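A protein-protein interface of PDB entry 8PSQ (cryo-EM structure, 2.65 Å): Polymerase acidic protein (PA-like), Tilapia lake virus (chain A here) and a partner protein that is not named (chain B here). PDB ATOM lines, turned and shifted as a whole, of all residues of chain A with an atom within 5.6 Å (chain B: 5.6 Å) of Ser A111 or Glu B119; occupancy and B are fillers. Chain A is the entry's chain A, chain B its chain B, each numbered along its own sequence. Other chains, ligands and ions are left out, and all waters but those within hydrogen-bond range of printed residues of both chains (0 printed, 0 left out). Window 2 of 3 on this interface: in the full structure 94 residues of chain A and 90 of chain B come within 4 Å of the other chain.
The backbone NH of Glu B119 lies close to the side-chain carboxylate of Glu B123, 3.2 Å away.
O of Leu B116 touches CE1 of His A108 (3.0 Å).
CB of Ala A110 touches O of Leu B116, 3.8 Å away.
Tyr A112 touches Leu B116.
Val B118 touches Tyr A112 (CG2 to CE2, 3.3 Å).
Tyr A112 touches Leu B121.
Leu B121 touches Glu A115 (CD1 to OE1, 3.0 Å).
O of Glu B119 lies within hydrogen-bond range of OG of Ser A111, at 2.7 Å.
OG of Ser A111 is in hydrogen-bond range of O of Val B118, 3.1 Å away.
Of the 8 printed residues of chain A, 5 touch a printed residue of chain B.
Hydrophobic or aromatic side chains of chain A that line the printed part of chain B: His A108, Ala A110 and Tyr A112.
Of the 7 printed residues of chain B, 4 touch a printed residue of chain A.
Of chain B, only Val B118 (3.1 Å) and Glu B119 (2.7 Å) come within 4 Å of Ser A111.
Printed residues of chain B within 4 Å of Tyr A112: Leu B116 (3.9 Å), Val B118 (3.3 Å) and Leu B121 (3.6 Å).
Of the printed residues of chain A, Leu B121 touches Tyr A112 (3.6 Å) and Glu A115 (3.0 Å).
Printed residues of chain B within 4 Å of Glu A115: Leu B121.
Of the printed residues of chain A, Val B118 touches Ser A111 (3.1 Å) and Tyr A112 (3.3 Å).
Printed residues of chain B within 4 Å of His A108: Leu B116 (3.0 Å).
The nearest residue of chain B that does not touch Ser A111 is Ser B120 (4.1 Å).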
ATOM      1  N   HIS A 108     -14.738  -6.492  15.911  1.00  0.00           N
ATOM      2  CA  HIS A 108     -15.967  -6.409  15.137  1.00  0.00           C
ATOM      3  C   HIS A 108     -17.139  -6.025  16.033  1.00  0.00           C
ATOM      4  O   HIS A 108     -17.319  -6.588  17.116  1.00  0.00           O
ATOM      5  CB  HIS A 108     -16.240  -7.745  14.451  1.00  0.00           C
ATOM      6  CG  HIS A 108     -17.551  -7.799  13.732  1.00  0.00           C
ATOM      7  ND1 HIS A 108     -18.732  -8.128  14.361  1.00  0.00           N
ATOM      8  CD2 HIS A 108     -17.868  -7.566  12.437  1.00  0.00           C
ATOM      9  CE1 HIS A 108     -19.719  -8.094  13.485  1.00  0.00           C
ATOM     10  NE2 HIS A 108     -19.222  -7.756  12.309  1.00  0.00           N
ATOM     11  N   LYS A 109     -17.941  -5.068  15.571  1.00  0.00           N
ATOM     12  CA  LYS A 109     -19.105  -4.593  16.313  1.00  0.00           C
ATOM     13  C   LYS A 109     -20.349  -5.270  15.754  1.00  0.00           C
ATOM     14  O   LYS A 109     -20.719  -5.051  14.596  1.00  0.00           O
ATOM     15  CB  LYS A 109     -19.222  -3.074  16.221  1.00  0.00           C
ATOM     16  CG  LYS A 109     -19.882  -2.433  17.430  1.00  0.00           C
ATOM     17  CD  LYS A 109     -20.199  -0.959  17.194  1.00  0.00           C
ATOM     18  CE  LYS A 109     -21.264  -0.750  16.121  1.00  0.00           C
ATOM     19  NZ  LYS A 109     -22.329  -1.792  16.129  1.00  0.00           N
ATOM     20  N   ALA A 110     -20.997  -6.089  16.577  1.00  0.00           N
ATOM     21  CA  ALA A 110     -22.198  -6.791  16.164  1.00  0.00           C
ATOM     22  C   ALA A 110     -23.392  -5.843  16.140  1.00  0.00           C
ATOM     23  O   ALA A 110     -23.366  -4.747  16.704  1.00  0.00           O
ATOM     24  CB  ALA A 110     -22.481  -7.965  17.099  1.00  0.00           C
ATOM     25  N   SER A 111     -24.456  -6.284  15.466  1.00  0.00           N
ATOM     26  CA  SER A 111     -25.667  -5.479  15.368  1.00  0.00           C
ATOM     27  C   SER A 111     -26.372  -5.321  16.709  1.00  0.00           C
ATOM     28  O   SER A 111     -27.182  -4.401  16.862  1.00  0.00           O
ATOM     29  CB  SER A 111     -26.625  -6.101  14.354  1.00  0.00           C
ATOM     30  OG  SER A 111     -27.280  -7.230  14.902  1.00  0.00           O
ATOM     31  N   TYR A 112     -26.085  -6.190  17.676  1.00  0.00           N
ATOM     32  CA  TYR A 112     -26.715  -6.154  18.988  1.00  0.00           C
ATOM     33  C   TYR A 112     -25.828  -5.515  20.048  1.00  0.00           C
ATOM     34  O   TYR A 112     -26.140  -5.608  21.240  1.00  0.00           O
ATOM     35  CB  TYR A 112     -27.106  -7.569  19.422  1.00  0.00           C
ATOM     36  CG  TYR A 112     -26.003  -8.591  19.255  1.00  0.00           C
ATOM     37  CD1 TYR A 112     -24.993  -8.712  20.197  1.00  0.00           C
ATOM     38  CD2 TYR A 112     -25.968  -9.427  18.150  1.00  0.00           C
ATOM     39  CE1 TYR A 112     -23.984  -9.638  20.047  1.00  0.00           C
ATOM     40  CE2 TYR A 112     -24.964 -10.355  17.992  1.00  0.00           C
ATOM     41  CZ  TYR A 112     -23.974 -10.457  18.942  1.00  0.00           C
ATOM     42  OH  TYR A 112     -22.971 -11.383  18.785  1.00  0.00           O
ATOM     43  N   ASP A 113     -24.732  -4.870  19.646  1.00  0.00           N
ATOM     44  CA  ASP A 113     -23.839  -4.246  20.618  1.00  0.00           C
ATOM     45  C   ASP A 113     -24.566  -3.201  21.453  1.00  0.00           C
ATOM     46  O   ASP A 113     -24.436  -3.177  22.683  1.00  0.00           O
ATOM     47  CB  ASP A 113     -22.652  -3.608  19.895  1.00  0.00           C
ATOM     48  CG  ASP A 113     -21.364  -3.720  20.678  1.00  0.00           C
ATOM     49  OD1 ASP A 113     -21.172  -2.927  21.623  1.00  0.00           O
ATOM     50  OD2 ASP A 113     -20.541  -4.598  20.350  1.00  0.00           O
ATOM     51  N   ALA A 114     -25.337  -2.328  20.802  1.00  0.00           N
ATOM     52  CA  ALA A 114     -25.989  -1.239  21.520  1.00  0.00           C
ATOM     53  C   ALA A 114     -26.986  -1.767  22.541  1.00  0.00           C
ATOM     54  O   ALA A 114     -27.068  -1.250  23.661  1.00  0.00           O
ATOM     55  CB  ALA A 114     -26.682  -0.304  20.530  1.00  0.00           C
ATOM     56  N   GLU A 115     -27.758  -2.790  22.173  1.00  0.00           N
ATOM     57  CA  GLU A 115     -28.743  -3.332  23.102  1.00  0.00           C
ATOM     58  C   GLU A 115     -28.074  -3.946  24.324  1.00  0.00           C
ATOM     59  O   GLU A 115     -28.529  -3.743  25.456  1.00  0.00           O
ATOM     60  CB  GLU A 115     -29.618  -4.363  22.394  1.00  0.00           C
ATOM     61  CG  GLU A 115     -30.878  -4.720  23.165  1.00  0.00           C
ATOM     62  CD  GLU A 115     -31.619  -5.893  22.563  1.00  0.00           C
ATOM     63  OE1 GLU A 115     -30.966  -6.749  21.934  1.00  0.00           O
ATOM     64  OE2 GLU A 115     -32.855  -5.961  22.725  1.00  0.00           O
ATOM     65  N   LEU B 116     -21.060 -13.601  15.897  1.00  0.00           N
ATOM     66  CA  LEU B 116     -20.772 -12.186  15.708  1.00  0.00           C
ATOM     67  C   LEU B 116     -21.489 -11.580  14.508  1.00  0.00           C
ATOM     68  O   LEU B 116     -21.495 -10.352  14.375  1.00  0.00           O
ATOM     69  CB  LEU B 116     -19.262 -11.978  15.555  1.00  0.00           C
ATOM     70  CG  LEU B 116     -18.467 -11.768  16.846  1.00  0.00           C
ATOM     71  CD1 LEU B 116     -16.976 -11.804  16.560  1.00  0.00           C
ATOM     72  CD2 LEU B 116     -18.853 -10.458  17.503  1.00  0.00           C
ATOM     73  N   THR B 117     -22.104 -12.392  13.650  1.00  0.00           N
ATOM     74  CA  THR B 117     -22.653 -11.940  12.376  1.00  0.00           C
ATOM     75  C   THR B 117     -24.123 -12.338  12.257  1.00  0.00           C
ATOM     76  O   THR B 117     -24.566 -12.893  11.250  1.00  0.00           O
ATOM     77  CB  THR B 117     -21.821 -12.497  11.217  1.00  0.00           C
ATOM     78  OG1 THR B 117     -20.534 -11.867  11.215  1.00  0.00           O
ATOM     79  CG2 THR B 117     -22.475 -12.224   9.862  1.00  0.00           C
ATOM     80  N   VAL B 118     -24.899 -12.070  13.302  1.00  0.00           N
ATOM     81  CA  VAL B 118     -26.338 -12.301  13.285  1.00  0.00           C
ATOM     82  C   VAL B 118     -27.043 -10.957  13.225  1.00  0.00           C
ATOM     83  O   VAL B 118     -26.504  -9.926  13.642  1.00  0.00           O
ATOM     84  CB  VAL B 118     -26.812 -13.118  14.509  1.00  0.00           C
ATOM     85  CG1 VAL B 118     -26.304 -14.538  14.414  1.00  0.00           C
ATOM     86  CG2 VAL B 118     -26.353 -12.470  15.806  1.00  0.00           C
ATOM     87  N   GLU B 119     -28.263 -10.965  12.685  1.00  0.00           N
ATOM     88  CA  GLU B 119     -29.032  -9.734  12.571  1.00  0.00           C
ATOM     89  C   GLU B 119     -29.646  -9.313  13.901  1.00  0.00           C
ATOM     90  O   GLU B 119     -29.729  -8.114  14.185  1.00  0.00           O
ATOM     91  CB  GLU B 119     -30.126  -9.898  11.514  1.00  0.00           C
ATOM     92  CG  GLU B 119     -29.601  -9.917  10.085  1.00  0.00           C
ATOM     93  CD  GLU B 119     -29.614 -11.305   9.476  1.00  0.00           C
ATOM     94  OE1 GLU B 119     -28.694 -12.096   9.775  1.00  0.00           O
ATOM     95  OE2 GLU B 119     -30.544 -11.605   8.699  1.00  0.00           O
ATOM     96  N   SER B 120     -30.068 -10.271  14.724  1.00  0.00           N
ATOM     97  CA  SER B 120     -30.691  -9.957  16.000  1.00  0.00           C
ATOM     98  C   SER B 120     -30.361 -11.057  16.995  1.00  0.00           C
ATOM     99  O   SER B 120     -29.933 -12.151  16.623  1.00  0.00           O
ATOM    100  CB  SER B 120     -32.210  -9.799  15.863  1.00  0.00           C
ATOM    101  OG  SER B 120     -32.789 -10.933  15.244  1.00  0.00           O
ATOM    102  N   LEU B 121     -30.564 -10.747  18.278  1.00  0.00           N
ATOM    103  CA  LEU B 121     -30.286 -11.720  19.327  1.00  0.00           C
ATOM    104  C   LEU B 121     -31.202 -12.932  19.230  1.00  0.00           C
ATOM    105  O   LEU B 121     -30.842 -14.016  19.697  1.00  0.00           O
ATOM    106  CB  LEU B 121     -30.429 -11.067  20.701  1.00  0.00           C
ATOM    107  CG  LEU B 121     -29.322 -10.100  21.124  1.00  0.00           C
ATOM    108  CD1 LEU B 121     -29.700  -9.411  22.418  1.00  0.00           C
ATOM    109  CD2 LEU B 121     -27.995 -10.819  21.277  1.00  0.00           C
ATOM    110  N   GLU B 123     -32.202 -14.353  16.394  1.00  0.00           N
ATOM    111  CA  GLU B 123     -31.938 -15.162  15.215  1.00  0.00           C
ATOM    112  C   GLU B 123     -31.346 -16.510  15.614  1.00  0.00           C
ATOM    113  O   GLU B 123     -30.541 -16.612  16.542  1.00  0.00           O
ATOM    114  CB  GLU B 123     -30.989 -14.432  14.268  1.00  0.00           C
ATOM    115  CG  GLU B 123     -30.685 -15.197  12.994  1.00  0.00           C
ATOM    116  CD  GLU B 123     -29.975 -14.346  11.963  1.00  0.00           C
ATOM    117  OE1 GLU B 123     -30.375 -13.178  11.784  1.00  0.00           O
ATOM    118  OE2 GLU B 123     -29.019 -14.844  11.334  1.00  0.00           O
